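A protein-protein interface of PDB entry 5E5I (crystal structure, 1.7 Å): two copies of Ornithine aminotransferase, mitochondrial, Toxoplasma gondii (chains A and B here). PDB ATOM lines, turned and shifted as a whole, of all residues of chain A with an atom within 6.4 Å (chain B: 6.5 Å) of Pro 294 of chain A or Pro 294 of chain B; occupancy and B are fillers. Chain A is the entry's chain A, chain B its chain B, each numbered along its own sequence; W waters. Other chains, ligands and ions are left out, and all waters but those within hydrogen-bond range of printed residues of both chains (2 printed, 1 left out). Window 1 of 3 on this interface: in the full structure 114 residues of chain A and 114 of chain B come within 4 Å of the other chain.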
ATOM      1  N   MET A 133      27.561  30.590  -4.364  1.00  0.00           N
ATOM      2  CA  MET A 133      26.452  31.103  -5.170  1.00  0.00           C
ATOM      3  C   MET A 133      25.284  30.151  -5.012  1.00  0.00           C
ATOM      4  O   MET A 133      25.273  29.290  -4.088  1.00  0.00           O
ATOM      5  CB  MET A 133      26.886  31.313  -6.640  1.00  0.00           C
ATOM      6  CG  MET A 133      27.931  32.403  -6.849  1.00  0.00           C
ATOM      7  SD  MET A 133      27.476  34.058  -6.426  1.00  0.00           S
ATOM      8  CE  MET A 133      26.345  34.550  -7.696  1.00  0.00           C
ATOM      9  N   ASN A 134      24.250  30.270  -5.861  1.00  0.00           N
ATOM     10  CA  ASN A 134      23.064  29.447  -5.592  1.00  0.00           C
ATOM     11  C   ASN A 134      22.866  28.339  -6.608  1.00  0.00           C
ATOM     12  O   ASN A 134      22.514  27.202  -6.263  1.00  0.00           O
ATOM     13  CB  ASN A 134      21.828  30.344  -5.488  1.00  0.00           C
ATOM     14  CG  ASN A 134      22.010  31.454  -4.492  1.00  0.00           C
ATOM     15  OD1 ASN A 134      21.855  31.245  -3.289  1.00  0.00           O
ATOM     16  ND2 ASN A 134      22.440  32.587  -4.951  1.00  0.00           N
ATOM     17  N   THR A 135      23.015  28.656  -7.857  1.00  0.00           N
ATOM     18  CA  THR A 135      22.792  27.662  -8.875  1.00  0.00           C
ATOM     19  C   THR A 135      24.066  27.364  -9.678  1.00  0.00           C
ATOM     20  O   THR A 135      25.035  28.111  -9.625  1.00  0.00           O
ATOM     21  CB  THR A 135      21.722  28.162  -9.851  1.00  0.00           C
ATOM     22  OG1 THR A 135      22.204  29.297 -10.622  1.00  0.00           O
ATOM     23  CG2 THR A 135      20.445  28.531  -9.137  1.00  0.00           C
ATOM     24  N   SER A 289      24.500  20.188  -1.998  1.00  0.00           N
ATOM     25  CA  SER A 289      23.435  20.311  -0.976  1.00  0.00           C
ATOM     26  C   SER A 289      22.598  19.038  -0.748  1.00  0.00           C
ATOM     27  O   SER A 289      21.560  19.124  -0.103  1.00  0.00           O
ATOM     28  CB  SER A 289      22.456  21.358  -1.459  1.00  0.00           C
ATOM     29  OG  SER A 289      21.709  20.849  -2.561  1.00  0.00           O
ATOM     30  N   GLY A 291      20.619  17.886  -2.814  1.00  0.00           N
ATOM     31  CA  GLY A 291      19.345  18.198  -3.484  1.00  0.00           C
ATOM     32  C   GLY A 291      18.341  18.867  -2.584  1.00  0.00           C
ATOM     33  O   GLY A 291      17.160  18.908  -2.911  1.00  0.00           O
ATOM     34  N   VAL A 292      18.795  19.438  -1.464  1.00  0.00           N
ATOM     35  CA  VAL A 292      17.901  20.035  -0.458  1.00  0.00           C
ATOM     36  C   VAL A 292      17.647  21.530  -0.683  1.00  0.00           C
ATOM     37  O   VAL A 292      16.510  21.988  -0.601  1.00  0.00           O
ATOM     38  CB  VAL A 292      18.406  19.715   0.960  1.00  0.00           C
ATOM     39  CG1 VAL A 292      17.588  20.434   2.029  1.00  0.00           C
ATOM     40  CG2 VAL A 292      18.436  18.213   1.215  1.00  0.00           C
ATOM     41  N   VAL A 293      18.670  22.280  -1.078  1.00  0.00           N
ATOM     42  CA  VAL A 293      18.478  23.688  -1.346  1.00  0.00           C
ATOM     43  C   VAL A 293      19.536  24.034  -2.389  1.00  0.00           C
ATOM     44  O   VAL A 293      20.598  23.434  -2.405  1.00  0.00           O
ATOM     45  CB  VAL A 293      18.634  24.499  -0.053  1.00  0.00           C
ATOM     46  CG1 VAL A 293      20.005  24.352   0.539  1.00  0.00           C
ATOM     47  CG2 VAL A 293      18.313  25.963  -0.236  1.00  0.00           C
ATOM     48  N   PRO A 294      19.275  25.044  -3.197  1.00  0.00           N
ATOM     49  CA  PRO A 294      20.298  25.370  -4.208  1.00  0.00           C
ATOM     50  C   PRO A 294      21.554  26.086  -3.642  1.00  0.00           C
ATOM     51  O   PRO A 294      21.453  27.167  -3.095  1.00  0.00           O
ATOM     52  CB  PRO A 294      19.571  26.294  -5.176  1.00  0.00           C
ATOM     53  CG  PRO A 294      18.283  26.620  -4.598  1.00  0.00           C
ATOM     54  CD  PRO A 294      18.000  25.754  -3.421  1.00  0.00           C
ATOM     55  N   ILE A 295      22.708  25.444  -3.718  1.00  0.00           N
ATOM     56  CA  ILE A 295      23.988  26.061  -3.302  1.00  0.00           C
ATOM     57  C   ILE A 295      25.033  25.564  -4.301  1.00  0.00           C
ATOM     58  O   ILE A 295      25.029  24.421  -4.685  1.00  0.00           O
ATOM     59  CB  ILE A 295      24.346  25.912  -1.797  1.00  0.00           C
ATOM     60  CG1 ILE A 295      25.765  26.398  -1.508  1.00  0.00           C
ATOM     61  CG2 ILE A 295      24.135  24.488  -1.278  1.00  0.00           C
ATOM     62  CD1 ILE A 295      26.068  26.665  -0.019  1.00  0.00           C
ATOM     63  N   SER A 296      25.799  26.504  -4.846  1.00  0.00           N
ATOM     64  CA  SER A 296      26.856  26.193  -5.778  1.00  0.00           C
ATOM     65  C   SER A 296      28.148  26.861  -5.274  1.00  0.00           C
ATOM     66  O   SER A 296      28.101  27.737  -4.407  1.00  0.00           O
ATOM     67  CB  SER A 296      26.506  26.674  -7.180  1.00  0.00           C
ATOM     68  OG  SER A 296      26.372  28.060  -7.149  1.00  0.00           O
ATOM     69  N   PHE A 317      21.224  35.495  -1.826  1.00  0.00           N
ATOM     70  CA  PHE A 317      21.252  34.242  -1.035  1.00  0.00           C
ATOM     71  C   PHE A 317      22.566  33.492  -1.047  1.00  0.00           C
ATOM     72  O   PHE A 317      22.683  32.478  -0.368  1.00  0.00           O
ATOM     73  CB  PHE A 317      20.148  33.305  -1.518  1.00  0.00           C
ATOM     74  CG  PHE A 317      18.771  33.697  -1.065  1.00  0.00           C
ATOM     75  CD1 PHE A 317      18.264  33.211   0.119  1.00  0.00           C
ATOM     76  CD2 PHE A 317      17.971  34.526  -1.855  1.00  0.00           C
ATOM     77  CE1 PHE A 317      16.992  33.570   0.530  1.00  0.00           C
ATOM     78  CE2 PHE A 317      16.694  34.898  -1.453  1.00  0.00           C
ATOM     79  CZ  PHE A 317      16.198  34.399  -0.235  1.00  0.00           C
ATOM     80  N   ASN A 320      24.265  31.837   2.214  1.00  0.00           N
ATOM     81  CA  ASN A 320      23.349  31.966   3.358  1.00  0.00           C
ATOM     82  C   ASN A 320      23.654  30.855   4.339  1.00  0.00           C
ATOM     83  O   ASN A 320      24.044  29.756   3.915  1.00  0.00           O
ATOM     84  CB  ASN A 320      21.883  32.009   2.909  1.00  0.00           C
ATOM     85  CG  ASN A 320      21.347  30.668   2.403  1.00  0.00           C
ATOM     86  OD1 ASN A 320      20.935  29.783   3.188  1.00  0.00           O
ATOM     87  ND2 ASN A 320      21.309  30.513   1.093  1.00  0.00           N
ATOM     88  N   ALA A 323      21.992  27.193   3.866  1.00  0.00           N
ATOM     89  CA  ALA A 323      22.598  26.401   2.804  1.00  0.00           C
ATOM     90  C   ALA A 323      23.995  25.926   3.195  1.00  0.00           C
ATOM     91  O   ALA A 323      24.376  24.853   2.830  1.00  0.00           O
ATOM     92  CB  ALA A 323      22.666  27.201   1.497  1.00  0.00           C
ATOM     93  N   MET B 133      12.129  30.112 -10.775  1.00  0.00           N
ATOM     94  CA  MET B 133      13.576  30.061 -10.840  1.00  0.00           C
ATOM     95  C   MET B 133      14.111  30.142  -9.403  1.00  0.00           C
ATOM     96  O   MET B 133      13.345  29.969  -8.431  1.00  0.00           O
ATOM     97  CB  MET B 133      14.161  31.133 -11.829  1.00  0.00           C
ATOM     98  CG  MET B 133      13.657  30.949 -13.280  1.00  0.00           C
ATOM     99  SD  MET B 133      14.234  29.441 -14.057  1.00  0.00           S
ATOM    100  CE  MET B 133      15.941  29.776 -14.298  1.00  0.00           C
ATOM    101  N   ASN B 134      15.425  30.288  -9.232  1.00  0.00           N
ATOM    102  CA  ASN B 134      15.989  30.289  -7.885  1.00  0.00           C
ATOM    103  C   ASN B 134      16.344  31.646  -7.357  1.00  0.00           C
ATOM    104  O   ASN B 134      16.053  31.949  -6.214  1.00  0.00           O
ATOM    105  CB  ASN B 134      17.194  29.323  -7.856  1.00  0.00           C
ATOM    106  CG  ASN B 134      16.852  28.025  -8.495  1.00  0.00           C
ATOM    107  OD1 ASN B 134      16.265  27.173  -7.856  1.00  0.00           O
ATOM    108  ND2 ASN B 134      17.151  27.884  -9.782  1.00  0.00           N
ATOM    109  N   THR B 135      16.960  32.489  -8.172  1.00  0.00           N
ATOM    110  CA  THR B 135      17.412  33.744  -7.699  1.00  0.00           C
ATOM    111  C   THR B 135      16.769  34.898  -8.480  1.00  0.00           C
ATOM    112  O   THR B 135      16.172  34.734  -9.546  1.00  0.00           O
ATOM    113  CB  THR B 135      18.949  33.868  -7.875  1.00  0.00           C
ATOM    114  OG1 THR B 135      19.291  33.904  -9.249  1.00  0.00           O
ATOM    115  CG2 THR B 135      19.678  32.715  -7.225  1.00  0.00           C
ATOM    116  N   SER B 289      10.215  33.667  -0.390  1.00  0.00           N
ATOM    117  CA  SER B 289      10.511  32.510   0.463  1.00  0.00           C
ATOM    118  C   SER B 289      10.679  32.853   1.949  1.00  0.00           C
ATOM    119  O   SER B 289      11.167  32.012   2.758  1.00  0.00           O
ATOM    120  CB  SER B 289      11.870  31.977   0.029  1.00  0.00           C
ATOM    121  OG  SER B 289      12.936  32.860   0.398  1.00  0.00           O
ATOM    122  N   GLY B 291      13.047  34.450   3.042  1.00  0.00           N
ATOM    123  CA  GLY B 291      14.481  34.392   3.270  1.00  0.00           C
ATOM    124  C   GLY B 291      15.013  33.062   3.719  1.00  0.00           C
ATOM    125  O   GLY B 291      16.160  32.967   4.239  1.00  0.00           O
ATOM    126  N   VAL B 292      14.211  32.022   3.491  1.00  0.00           N
ATOM    127  CA  VAL B 292      14.555  30.676   3.957  1.00  0.00           C
ATOM    128  C   VAL B 292      15.346  29.893   2.910  1.00  0.00           C
ATOM    129  O   VAL B 292      16.342  29.244   3.258  1.00  0.00           O
ATOM    130  CB  VAL B 292      13.304  29.965   4.495  1.00  0.00           C
ATOM    131  CG1 VAL B 292      13.611  28.550   4.894  1.00  0.00           C
ATOM    132  CG2 VAL B 292      12.738  30.740   5.651  1.00  0.00           C
ATOM    133  N   VAL B 293      14.928  29.972   1.654  1.00  0.00           N
ATOM    134  CA  VAL B 293      15.612  29.317   0.558  1.00  0.00           C
ATOM    135  C   VAL B 293      15.421  30.199  -0.678  1.00  0.00           C
ATOM    136  O   VAL B 293      14.428  30.938  -0.796  1.00  0.00           O
ATOM    137  CB  VAL B 293      15.081  27.929   0.215  1.00  0.00           C
ATOM    138  CG1 VAL B 293      15.303  26.923   1.350  1.00  0.00           C
ATOM    139  CG2 VAL B 293      13.601  27.998  -0.099  1.00  0.00           C
ATOM    140  N   PRO B 294      16.300  30.048  -1.647  1.00  0.00           N
ATOM    141  CA  PRO B 294      16.178  30.918  -2.837  1.00  0.00           C
ATOM    142  C   PRO B 294      15.095  30.456  -3.842  1.00  0.00           C
ATOM    143  O   PRO B 294      15.138  29.370  -4.291  1.00  0.00           O
ATOM    144  CB  PRO B 294      17.545  30.836  -3.504  1.00  0.00           C
ATOM    145  CG  PRO B 294      18.380  29.980  -2.648  1.00  0.00           C
ATOM    146  CD  PRO B 294      17.585  29.331  -1.582  1.00  0.00           C
ATOM    147  N   ILE B 295      14.073  31.260  -4.060  1.00  0.00           N
ATOM    148  CA  ILE B 295      13.030  30.970  -5.036  1.00  0.00           C
ATOM    149  C   ILE B 295      12.569  32.294  -5.596  1.00  0.00           C
ATOM    150  O   ILE B 295      12.340  33.204  -4.847  1.00  0.00           O
ATOM    151  CB  ILE B 295      11.841  30.124  -4.500  1.00  0.00           C
ATOM    152  CG1 ILE B 295      10.670  30.081  -5.514  1.00  0.00           C
ATOM    153  CG2 ILE B 295      11.418  30.592  -3.147  1.00  0.00           C
ATOM    154  CD1 ILE B 295       9.664  28.976  -5.256  1.00  0.00           C
ATOM    155  N   SER B 296      12.561  32.395  -6.926  1.00  0.00           N
ATOM    156  CA  SER B 296      12.086  33.587  -7.599  1.00  0.00           C
ATOM    157  C   SER B 296      10.991  33.159  -8.609  1.00  0.00           C
ATOM    158  O   SER B 296      10.803  31.962  -8.898  1.00  0.00           O
ATOM    159  CB  SER B 296      13.276  34.248  -8.253  1.00  0.00           C
ATOM    160  OG  SER B 296      13.781  33.367  -9.214  1.00  0.00           O
ATOM    161  N   PHE B 317      17.135  23.366  -9.904  1.00  0.00           N
ATOM    162  CA  PHE B 317      16.366  23.600  -8.663  1.00  0.00           C
ATOM    163  C   PHE B 317      15.091  24.406  -8.815  1.00  0.00           C
ATOM    164  O   PHE B 317      14.326  24.534  -7.863  1.00  0.00           O
ATOM    165  CB  PHE B 317      17.265  24.198  -7.561  1.00  0.00           C
ATOM    166  CG  PHE B 317      18.213  23.180  -6.917  1.00  0.00           C
ATOM    167  CD1 PHE B 317      17.822  22.460  -5.825  1.00  0.00           C
ATOM    168  CD2 PHE B 317      19.470  22.944  -7.421  1.00  0.00           C
ATOM    169  CE1 PHE B 317      18.664  21.504  -5.266  1.00  0.00           C
ATOM    170  CE2 PHE B 317      20.332  21.997  -6.863  1.00  0.00           C
ATOM    171  CZ  PHE B 317      19.915  21.274  -5.759  1.00  0.00           C
ATOM    172  N   ASN B 320      11.506  23.503  -7.341  1.00  0.00           N
ATOM    173  CA  ASN B 320      11.652  22.312  -6.517  1.00  0.00           C
ATOM    174  C   ASN B 320      10.544  22.315  -5.464  1.00  0.00           C
ATOM    175  O   ASN B 320      10.171  23.376  -4.983  1.00  0.00           O
ATOM    176  CB  ASN B 320      13.040  22.160  -5.868  1.00  0.00           C
ATOM    177  CG  ASN B 320      13.328  23.185  -4.775  1.00  0.00           C
ATOM    178  OD1 ASN B 320      12.971  22.986  -3.588  1.00  0.00           O
ATOM    179  ND2 ASN B 320      14.059  24.267  -5.134  1.00  0.00           N
ATOM    180  N   ALA B 323      11.075  24.376  -1.993  1.00  0.00           N
ATOM    181  CA  ALA B 323      10.921  25.805  -2.117  1.00  0.00           C
ATOM    182  C   ALA B 323       9.471  26.227  -2.346  1.00  0.00           C
ATOM    183  O   ALA B 323       9.048  27.265  -1.839  1.00  0.00           O
ATOM    184  CB  ALA B 323      11.773  26.346  -3.260  1.00  0.00           C
HETATM  185  O   HOH W   1      14.978  23.994  -1.910  1.00  0.00           O
HETATM  186  O   HOH W   2      18.700  28.451   1.985  1.00  0.00           O
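Water W2 bridges O of Val 292 of chain B and OD1 of Asn 320 of chain A.
Water W1 bridges OD1 of Asn 320 of chain B (2.8 Å) and O of Val 292 of chain A (2.8 Å).
Among the printed residues, pairs that only touch across the chains: Thr 135 of chain A with Asn 134 of chain B, Val 293 of chain A with Val 293 of chain B, Asn 134 of chain A with Thr 135 of chain B, Phe 317 of chain A with Ser 289 of chain B, Ser 289 of chain A with Phe 317 of chain B, Val 293 of chain A with Pro 294 of chain B, Asn 134 of chain A with Pro 294 of chain B, Gly 291 of chain A with Phe 317 of chain B, Phe 317 of chain A with Gly 291 of chain B, Pro 294 of chain A with Phe 317 of chain B, Pro 294 of chain A with Asn 134 of chain B, Pro 294 of chain A with Pro 294 of chain B, Phe 317 of chain A with Val 293 of chain B, Val 293 of chain A with Phe 317 of chain B and Phe 317 of chain A with Pro 294 of chain B.
The backbone carbonyl oxygen of Val 293 of chain B sits at hydrogen-bond distance from the side-chain hydroxyl of Ser 289 of chain B (2.7 Å).
The backbone carbonyl oxygen (O) of Thr 135 of chain B is in hydrogen-bond range of the side-chain hydroxyl (OG) of Ser 296 of chain B, 2.8 Å away.
O of Phe 317 of chain A sits at hydrogen-bond distance from ND2 of Asn 320 of chain A.
The side-chain hydroxyl of Ser 289 of chain B is in hydrogen-bond range of the backbone NH of Val 292 of chain B (3.4 Å).
The side-chain hydroxyl of Ser 289 of chain A is in hydrogen-bond range of the backbone NH of Val 292 of chain A, 3.4 Å away.
The side-chain hydroxyl of Ser 289 of chain B lies close to the backbone NH of Gly 291 of chain B, 3.1 Å away.
Printed residues of chain B that touch a printed residue of chain A: Asn 134, Thr 135, Ser 289, Gly 291, Val 293, Pro 294 and Phe 317.
Of the 13 printed residues of chain A, 7 touch a printed residue of chain B.
Among the printed residues, no Asp or Glu carboxylate lies within 4 Å of a Lys or Arg side-chain nitrogen of the other chain.
Of chain B, only Asn 134, Pro 294 and Phe 317 come within 4 Å of Pro 294 of chain A.
Printed residues of chain A within 4 Å of Pro 294 of chain B: Asn 134 (3.8 Å), Val 293 (3.7 Å), Pro 294 (3.9 Å) and Phe 317 (3.9 Å).
Of the printed residues of chain A, Phe 317 of chain B touches Ser 289, Gly 291, Val 293 and Pro 294.
Of the printed residues of chain A, Asn 134 of chain B touches Thr 135 and Pro 294.
Of the printed residues of chain B, Phe 317 of chain A touches Ser 289, Gly 291, Val 293 and Pro 294.
Printed residues of chain B within 4 Å of Asn 134 of chain A: Thr 135 (3.6 Å) and Pro 294 (3.8 Å).
Met 133 of chain A touches none of the printed residues of chain B.
Asn 134 of chain A touches Pro 294 of chain B, and with the chains exchanged Pro 294 of chain A touches Asn 134 of chain B.
Val 293 of chain B touches its own counterpart, Val 293 of chain A.
Val 293 of chain A touches Phe 317 of chain B, and with the chains exchanged Phe 317 of chain A touches Val 293 of chain B.
Pro 294 of chain A touches Phe 317 of chain B, and with the chains exchanged Phe 317 of chain A touches Pro 294 of chain B.
Positions printed for both chains: 133, 134, 135, 289, 291, 292, 293, 294, 295, 296, 317, 320 and 323.
Of the 15 pairs that touch across the chains among the printed residues, 14 have their exchanged pair printed and touching as well.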
